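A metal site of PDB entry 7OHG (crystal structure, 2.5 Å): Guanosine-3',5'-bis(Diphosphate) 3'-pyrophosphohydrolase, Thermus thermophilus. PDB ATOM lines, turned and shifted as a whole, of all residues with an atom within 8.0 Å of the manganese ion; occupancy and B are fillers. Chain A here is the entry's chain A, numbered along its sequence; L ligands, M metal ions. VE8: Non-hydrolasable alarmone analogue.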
ATOM      1  N   HIS A  38       0.469  16.555  39.860  1.00  0.00           N
ATOM      2  CA  HIS A  38       0.033  15.308  39.220  1.00  0.00           C
ATOM      3  C   HIS A  38       0.848  14.084  39.654  1.00  0.00           C
ATOM      4  O   HIS A  38       0.835  13.083  38.933  1.00  0.00           O
ATOM      5  CB  HIS A  38       0.109  15.448  37.683  1.00  0.00           C
ATOM      6  CG  HIS A  38      -0.838  16.461  37.114  1.00  0.00           C
ATOM      7  ND1 HIS A  38      -2.199  16.283  37.187  1.00  0.00           N
ATOM      8  CD2 HIS A  38      -0.578  17.606  36.451  1.00  0.00           C
ATOM      9  CE1 HIS A  38      -2.727  17.341  36.586  1.00  0.00           C
ATOM     10  NE2 HIS A  38      -1.787  18.159  36.127  1.00  0.00           N
ATOM     11  N   ARG A  43      -2.141   8.401  33.227  1.00  0.00           N
ATOM     12  CA  ARG A  43      -2.981   8.514  32.068  1.00  0.00           C
ATOM     13  C   ARG A  43      -3.387   7.105  31.660  1.00  0.00           C
ATOM     14  O   ARG A  43      -2.692   6.149  31.976  1.00  0.00           O
ATOM     15  CB  ARG A  43      -2.221   9.206  30.938  1.00  0.00           C
ATOM     16  CG  ARG A  43      -2.297  10.714  31.035  1.00  0.00           C
ATOM     17  CD  ARG A  43      -2.290  11.324  29.669  1.00  0.00           C
ATOM     18  NE  ARG A  43      -3.462  12.169  29.434  1.00  0.00           N
ATOM     19  CZ  ARG A  43      -3.824  12.625  28.234  1.00  0.00           C
ATOM     20  NH1 ARG A  43      -4.892  13.397  28.103  1.00  0.00           N
ATOM     21  NH2 ARG A  43      -3.119  12.302  27.148  1.00  0.00           N
ATOM     22  N   TYR A  49       0.668  11.116  34.521  1.00  0.00           N
ATOM     23  CA  TYR A  49      -0.152  12.218  34.019  1.00  0.00           C
ATOM     24  C   TYR A  49       0.619  13.403  33.412  1.00  0.00           C
ATOM     25  O   TYR A  49       0.235  13.899  32.346  1.00  0.00           O
ATOM     26  CB  TYR A  49      -1.135  12.727  35.067  1.00  0.00           C
ATOM     27  CG  TYR A  49      -2.325  13.381  34.404  1.00  0.00           C
ATOM     28  CD1 TYR A  49      -3.307  12.609  33.783  1.00  0.00           C
ATOM     29  CD2 TYR A  49      -2.404  14.761  34.274  1.00  0.00           C
ATOM     30  CE1 TYR A  49      -4.365  13.204  33.113  1.00  0.00           C
ATOM     31  CE2 TYR A  49      -3.455  15.365  33.587  1.00  0.00           C
ATOM     32  CZ  TYR A  49      -4.447  14.580  33.028  1.00  0.00           C
ATOM     33  OH  TYR A  49      -5.484  15.159  32.333  1.00  0.00           O
ATOM     34  N   HIS A  52       0.992  14.447  29.650  1.00  0.00           N
ATOM     35  CA  HIS A  52      -0.015  15.243  28.975  1.00  0.00           C
ATOM     36  C   HIS A  52       0.247  16.758  29.070  1.00  0.00           C
ATOM     37  O   HIS A  52       0.510  17.342  28.012  1.00  0.00           O
ATOM     38  CB  HIS A  52      -1.427  14.850  29.435  1.00  0.00           C
ATOM     39  CG  HIS A  52      -2.546  15.753  28.986  1.00  0.00           C
ATOM     40  ND1 HIS A  52      -2.841  15.934  27.657  1.00  0.00           N
ATOM     41  CD2 HIS A  52      -3.473  16.418  29.727  1.00  0.00           C
ATOM     42  CE1 HIS A  52      -3.911  16.722  27.620  1.00  0.00           C
ATOM     43  NE2 HIS A  52      -4.322  17.033  28.844  1.00  0.00           N
ATOM     44  N   PRO A  53       0.273  17.439  30.248  1.00  0.00           N
ATOM     45  CA  PRO A  53       0.501  18.889  30.233  1.00  0.00           C
ATOM     46  C   PRO A  53       1.860  19.305  29.688  1.00  0.00           C
ATOM     47  O   PRO A  53       1.988  20.431  29.211  1.00  0.00           O
ATOM     48  CB  PRO A  53       0.274  19.304  31.680  1.00  0.00           C
ATOM     49  CG  PRO A  53      -0.554  18.224  32.268  1.00  0.00           C
ATOM     50  CD  PRO A  53      -0.022  16.976  31.612  1.00  0.00           C
ATOM     51  N   VAL A  56       1.037  19.232  25.927  1.00  0.00           N
ATOM     52  CA  VAL A  56       0.201  20.400  25.674  1.00  0.00           C
ATOM     53  C   VAL A  56       1.036  21.695  25.678  1.00  0.00           C
ATOM     54  O   VAL A  56       0.887  22.506  24.763  1.00  0.00           O
ATOM     55  CB  VAL A  56      -1.006  20.457  26.623  1.00  0.00           C
ATOM     56  CG1 VAL A  56      -1.816  21.723  26.397  1.00  0.00           C
ATOM     57  CG2 VAL A  56      -1.886  19.230  26.440  1.00  0.00           C
ATOM     58  N   GLY A  73      -0.401  25.988  30.033  1.00  0.00           N
ATOM     59  CA  GLY A  73      -0.501  24.696  29.362  1.00  0.00           C
ATOM     60  C   GLY A  73       0.017  23.581  30.245  1.00  0.00           C
ATOM     61  O   GLY A  73      -0.526  22.471  30.226  1.00  0.00           O
ATOM     62  N   HIS A  76      -2.768  23.530  33.206  1.00  0.00           N
ATOM     63  CA  HIS A  76      -4.164  23.476  32.781  1.00  0.00           C
ATOM     64  C   HIS A  76      -4.982  22.340  33.381  1.00  0.00           C
ATOM     65  O   HIS A  76      -6.181  22.344  33.197  1.00  0.00           O
ATOM     66  CB  HIS A  76      -4.268  23.460  31.239  1.00  0.00           C
ATOM     67  CG  HIS A  76      -4.152  22.109  30.621  1.00  0.00           C
ATOM     68  ND1 HIS A  76      -2.959  21.414  30.629  1.00  0.00           N
ATOM     69  CD2 HIS A  76      -5.089  21.353  30.018  1.00  0.00           C
ATOM     70  CE1 HIS A  76      -3.205  20.273  30.022  1.00  0.00           C
ATOM     71  NE2 HIS A  76      -4.476  20.185  29.647  1.00  0.00           N
ATOM     72  N   ASP A  77      -4.360  21.374  34.098  1.00  0.00           N
ATOM     73  CA  ASP A  77      -5.127  20.276  34.692  1.00  0.00           C
ATOM     74  C   ASP A  77      -5.083  20.245  36.218  1.00  0.00           C
ATOM     75  O   ASP A  77      -5.955  19.624  36.824  1.00  0.00           O
ATOM     76  CB  ASP A  77      -4.715  18.923  34.109  1.00  0.00           C
ATOM     77  CG  ASP A  77      -5.447  18.529  32.851  1.00  0.00           C
ATOM     78  OD1 ASP A  77      -6.692  18.689  32.803  1.00  0.00           O
ATOM     79  OD2 ASP A  77      -4.780  18.017  31.903  1.00  0.00           O
ATOM     80  N   THR A  78      -4.141  20.972  36.809  1.00  0.00           N
ATOM     81  CA  THR A  78      -3.876  20.977  38.272  1.00  0.00           C
ATOM     82  C   THR A  78      -5.085  21.284  39.159  1.00  0.00           C
ATOM     83  O   THR A  78      -5.148  20.731  40.250  1.00  0.00           O
ATOM     84  CB  THR A  78      -2.813  22.039  38.535  1.00  0.00           C
ATOM     85  OG1 THR A  78      -3.295  23.277  38.027  1.00  0.00           O
ATOM     86  CG2 THR A  78      -1.480  21.693  37.902  1.00  0.00           C
ATOM     87  N   ASP A  81      -7.830  17.851  39.584  1.00  0.00           N
ATOM     88  CA  ASP A  81      -7.333  16.602  40.154  1.00  0.00           C
ATOM     89  C   ASP A  81      -6.585  16.631  41.530  1.00  0.00           C
ATOM     90  O   ASP A  81      -6.653  15.645  42.254  1.00  0.00           O
ATOM     91  CB  ASP A  81      -6.392  15.869  39.127  1.00  0.00           C
ATOM     92  CG  ASP A  81      -6.657  15.926  37.613  1.00  0.00           C
ATOM     93  OD1 ASP A  81      -7.048  17.003  37.096  1.00  0.00           O
ATOM     94  OD2 ASP A  81      -6.382  14.887  36.916  1.00  0.00           O
ATOM     95  N   GLU A 104      -9.857  27.203  30.596  1.00  0.00           N
ATOM     96  CA  GLU A 104      -9.761  25.960  29.819  1.00  0.00           C
ATOM     97  C   GLU A 104     -10.515  24.868  30.568  1.00  0.00           C
ATOM     98  O   GLU A 104     -11.223  24.076  29.926  1.00  0.00           O
ATOM     99  CB  GLU A 104      -8.303  25.532  29.577  1.00  0.00           C
ATOM    100  CG  GLU A 104      -8.135  24.259  28.756  1.00  0.00           C
ATOM    101  CD  GLU A 104      -8.067  22.930  29.492  1.00  0.00           C
ATOM    102  OE1 GLU A 104      -7.619  22.919  30.664  1.00  0.00           O
ATOM    103  OE2 GLU A 104      -8.475  21.896  28.917  1.00  0.00           O
ATOM    104  N   THR A 105     -10.370  24.806  31.905  1.00  0.00           N
ATOM    105  CA  THR A 105     -11.043  23.744  32.646  1.00  0.00           C
ATOM    106  C   THR A 105     -12.555  23.956  32.749  1.00  0.00           C
ATOM    107  O   THR A 105     -13.294  22.968  32.769  1.00  0.00           O
ATOM    108  CB  THR A 105     -10.416  23.492  34.025  1.00  0.00           C
ATOM    109  OG1 THR A 105     -10.916  24.412  35.008  1.00  0.00           O
ATOM    110  CG2 THR A 105      -8.904  23.476  34.001  1.00  0.00           C
ATOM    111  N   SER A 108     -14.833  22.972  29.483  1.00  0.00           N
ATOM    112  CA  SER A 108     -14.927  21.514  29.323  1.00  0.00           C
ATOM    113  C   SER A 108     -16.284  20.980  29.806  1.00  0.00           C
ATOM    114  O   SER A 108     -16.910  20.153  29.145  1.00  0.00           O
ATOM    115  CB  SER A 108     -13.778  20.844  30.080  1.00  0.00           C
ATOM    116  OG  SER A 108     -12.520  21.440  29.805  1.00  0.00           O
ATOM    117  N   VAL A 142      -5.397  27.134  24.411  1.00  0.00           N
ATOM    118  CA  VAL A 142      -4.989  26.102  25.374  1.00  0.00           C
ATOM    119  C   VAL A 142      -5.925  24.911  25.282  1.00  0.00           C
ATOM    120  O   VAL A 142      -5.461  23.772  25.178  1.00  0.00           O
ATOM    121  CB  VAL A 142      -4.792  26.642  26.798  1.00  0.00           C
ATOM    122  CG1 VAL A 142      -4.286  25.553  27.726  1.00  0.00           C
ATOM    123  CG2 VAL A 142      -3.802  27.789  26.781  1.00  0.00           C
ATOM    124  N   LYS A 143      -7.248  25.173  25.192  1.00  0.00           N
ATOM    125  CA  LYS A 143      -8.245  24.131  25.006  1.00  0.00           C
ATOM    126  C   LYS A 143      -8.039  23.371  23.670  1.00  0.00           C
ATOM    127  O   LYS A 143      -8.258  22.157  23.609  1.00  0.00           O
ATOM    128  CB  LYS A 143      -9.657  24.737  25.047  1.00  0.00           C
ATOM    129  CG  LYS A 143     -10.771  23.681  25.020  1.00  0.00           C
ATOM    130  CD  LYS A 143     -10.739  22.758  26.262  1.00  0.00           C
ATOM    131  CE  LYS A 143     -11.383  21.414  26.049  1.00  0.00           C
ATOM    132  NZ  LYS A 143     -11.285  20.587  27.274  1.00  0.00           N
ATOM    133  N   ALA A 145      -5.072  23.048  22.103  1.00  0.00           N
ATOM    134  CA  ALA A 145      -3.816  22.307  22.286  1.00  0.00           C
ATOM    135  C   ALA A 145      -4.055  21.061  23.124  1.00  0.00           C
ATOM    136  O   ALA A 145      -3.410  20.036  22.905  1.00  0.00           O
ATOM    137  CB  ALA A 145      -2.787  23.200  22.968  1.00  0.00           C
ATOM    138  N   ASP A 146      -4.969  21.154  24.091  1.00  0.00           N
ATOM    139  CA  ASP A 146      -5.347  20.074  24.955  1.00  0.00           C
ATOM    140  C   ASP A 146      -6.078  19.042  24.114  1.00  0.00           C
ATOM    141  O   ASP A 146      -5.698  17.865  24.146  1.00  0.00           O
ATOM    142  CB  ASP A 146      -6.242  20.607  26.104  1.00  0.00           C
ATOM    143  CG  ASP A 146      -6.995  19.561  26.927  1.00  0.00           C
ATOM    144  OD1 ASP A 146      -6.391  18.991  27.871  1.00  0.00           O
ATOM    145  OD2 ASP A 146      -8.201  19.348  26.649  1.00  0.00           O
ATOM    146  N   ARG A 147      -7.086  19.480  23.321  1.00  0.00           N
ATOM    147  CA  ARG A 147      -7.861  18.567  22.475  1.00  0.00           C
ATOM    148  C   ARG A 147      -6.975  17.900  21.446  1.00  0.00           C
ATOM    149  O   ARG A 147      -7.161  16.721  21.174  1.00  0.00           O
ATOM    150  CB  ARG A 147      -9.053  19.267  21.811  1.00  0.00           C
ATOM    151  CG  ARG A 147      -9.809  18.428  20.757  1.00  0.00           C
ATOM    152  CD  ARG A 147     -10.366  17.123  21.311  1.00  0.00           C
ATOM    153  NE  ARG A 147     -11.210  17.311  22.494  1.00  0.00           N
ATOM    154  CZ  ARG A 147     -12.545  17.361  22.469  1.00  0.00           C
ATOM    155  NH1 ARG A 147     -13.204  17.212  21.325  1.00  0.00           N
ATOM    156  NH2 ARG A 147     -13.224  17.557  23.596  1.00  0.00           N
ATOM    157  N   HIS A 149      -3.670  17.129  21.766  1.00  0.00           N
ATOM    158  CA  HIS A 149      -2.901  16.088  22.399  1.00  0.00           C
ATOM    159  C   HIS A 149      -3.733  14.893  22.754  1.00  0.00           C
ATOM    160  O   HIS A 149      -3.268  13.770  22.561  1.00  0.00           O
ATOM    161  CB  HIS A 149      -2.128  16.570  23.625  1.00  0.00           C
ATOM    162  CG  HIS A 149      -1.186  15.505  24.128  1.00  0.00           C
ATOM    163  ND1 HIS A 149      -1.286  15.008  25.390  1.00  0.00           N
ATOM    164  CD2 HIS A 149      -0.219  14.836  23.463  1.00  0.00           C
ATOM    165  CE1 HIS A 149      -0.333  14.099  25.481  1.00  0.00           C
ATOM    166  NE2 HIS A 149       0.319  13.955  24.333  1.00  0.00           N
ATOM    167  N   ASN A 150      -4.973  15.111  23.202  1.00  0.00           N
ATOM    168  CA  ASN A 150      -5.907  14.036  23.526  1.00  0.00           C
ATOM    169  C   ASN A 150      -6.161  13.176  22.296  1.00  0.00           C
ATOM    170  O   ASN A 150      -6.191  11.958  22.403  1.00  0.00           O
ATOM    171  CB  ASN A 150      -7.235  14.601  24.022  1.00  0.00           C
ATOM    172  CG  ASN A 150      -7.238  15.110  25.449  1.00  0.00           C
ATOM    173  OD1 ASN A 150      -6.527  14.609  26.343  1.00  0.00           O
ATOM    174  ND2 ASN A 150      -8.065  16.116  25.698  1.00  0.00           N
HETATM  175  O17 VE8 L   1     -14.554  11.052  29.506  1.00  0.00           O
HETATM  176  P2  VE8 L   1     -13.930  12.323  29.927  1.00  0.00           P
HETATM  177  O9  VE8 L   1     -14.876  13.523  29.994  1.00  0.00           O
HETATM  178  O10 VE8 L   1     -13.228  12.196  31.357  1.00  0.00           O
HETATM  179  P3  VE8 L   1     -13.453  11.311  32.662  1.00  0.00           P
HETATM  180  O16 VE8 L   1     -14.138  12.093  33.721  1.00  0.00           O
HETATM  181  O15 VE8 L   1     -14.167  10.014  32.224  1.00  0.00           O
HETATM  182  O11 VE8 L   1     -11.956  10.917  33.089  1.00  0.00           O
HETATM  183  P4  VE8 L   1     -11.253   9.915  34.128  1.00  0.00           P
HETATM  184  O14 VE8 L   1     -11.546   8.485  33.783  1.00  0.00           O
HETATM  185  O13 VE8 L   1     -11.773  10.343  35.511  1.00  0.00           O
HETATM  186  O12 VE8 L   1      -9.751  10.262  34.037  1.00  0.00           O
HETATM  187  O8  VE8 L   1     -12.753  12.736  28.908  1.00  0.00           O
HETATM  188  C7  VE8 L   1     -11.617  11.915  28.556  1.00  0.00           C
HETATM  189  C6  VE8 L   1     -10.496  12.160  29.532  1.00  0.00           C
HETATM  190  C5  VE8 L   1      -9.650  13.417  29.302  1.00  0.00           C
HETATM  191  N1  VE8 L   1     -10.126  14.626  30.023  1.00  0.00           N
HETATM  192  P   VE8 L   1      -9.815  16.206  29.651  1.00  0.00           P
HETATM  193  O7  VE8 L   1      -9.999  17.123  30.775  1.00  0.00           O
HETATM  194  O6  VE8 L   1      -8.286  16.304  29.245  1.00  0.00           O
HETATM  195  O2  VE8 L   1     -10.700  16.684  28.362  1.00  0.00           O
HETATM  196  P1  VE8 L   1     -12.225  16.633  27.868  1.00  0.00           P
HETATM  197  O5  VE8 L   1     -12.425  15.622  26.765  1.00  0.00           O
HETATM  198  O4  VE8 L   1     -13.051  16.339  29.144  1.00  0.00           O
HETATM  199  O3  VE8 L   1     -12.529  18.074  27.401  1.00  0.00           O
HETATM  200  C4  VE8 L   1      -8.174  12.982  29.527  1.00  0.00           C
HETATM  201  O1  VE8 L   1      -7.506  13.797  30.480  1.00  0.00           O
HETATM  202  O18 VE8 L   1      -9.546  11.080  29.458  1.00  0.00           O
HETATM  203  C3  VE8 L   1      -8.331  11.530  29.999  1.00  0.00           C
HETATM  204  N   VE8 L   1      -7.251  10.625  29.565  1.00  0.00           N
HETATM  205  C8  VE8 L   1      -6.457   9.854  30.377  1.00  0.00           C
HETATM  206  N2  VE8 L   1      -5.591   9.125  29.708  1.00  0.00           N
HETATM  207  C1  VE8 L   1      -5.833   9.434  28.387  1.00  0.00           C
HETATM  208  C2  VE8 L   1      -6.849  10.354  28.274  1.00  0.00           C
HETATM  209  N3  VE8 L   1      -7.351  10.901  27.156  1.00  0.00           N
HETATM  210  C9  VE8 L   1      -6.753  10.463  26.047  1.00  0.00           C
HETATM  211  N4  VE8 L   1      -7.167  10.900  24.862  1.00  0.00           N
HETATM  212  N5  VE8 L   1      -5.737   9.552  26.055  1.00  0.00           N
HETATM  213  C   VE8 L   1      -5.197   8.974  27.185  1.00  0.00           C
HETATM  214  O   VE8 L   1      -4.285   8.157  27.099  1.00  0.00           O
HETATM  215 MN    MN M   1      -6.244  18.188  29.776  1.00  0.00          MN
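The side-chain hydroxyl (OH) of Tyr 49 lies within hydrogen-bond range of an oxygen (O1) of the ligand, at 3.1 Å. The backbone carbonyl oxygen (O) of Asn 150 is in hydrogen-bond range of a nitrogen (N4) of the ligand, at 2.8 Å. NZ of Lys 143 is in salt-bridge range of O3 of the ligand (2.8 Å). The guanidinium group of Arg 147 is in salt-bridge range of an oxygen (O5) of the ligand (3.8 Å).
O of Asp 146 is in hydrogen-bond range of ND2 of Asn 150 (3.3 Å). The side-chain carboxylate of Asp 146 lies within salt-bridge range of the side-chain amino group of Lys 143, 3.4 Å away. A ring nitrogen (ND1) of His 52 is in hydrogen-bond range of the guanidinium group (NH1) of Arg 43, at 3.3 Å. A ring nitrogen (ND1) of His 52 is in hydrogen-bond range of a ring nitrogen (ND1) of His 149 (2.9 Å). OD2 of Asp 77 sits close to OH of Tyr 49, 3.0 Å away. A ring nitrogen (ND1) of His 76 sits at hydrogen-bond distance from the backbone carbonyl oxygen of Gly 73 (2.7 Å).
Within 4 Å of the manganese ion: His 52, His 76, Asp 77 and Asp 146.
The manganese ion is bound by OD1 of Asp 146 (2.1 Å). NE2 of His 52 binds the manganese ion, at 2.4 Å. OD2 of Asp 77 binds the manganese ion (2.6 Å). The manganese ion is bound by a ring nitrogen (NE2) of His 76, 2.7 Å away. Slightly farther from the manganese ion lies an oxygen (O6) of the ligand (2.8 Å).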
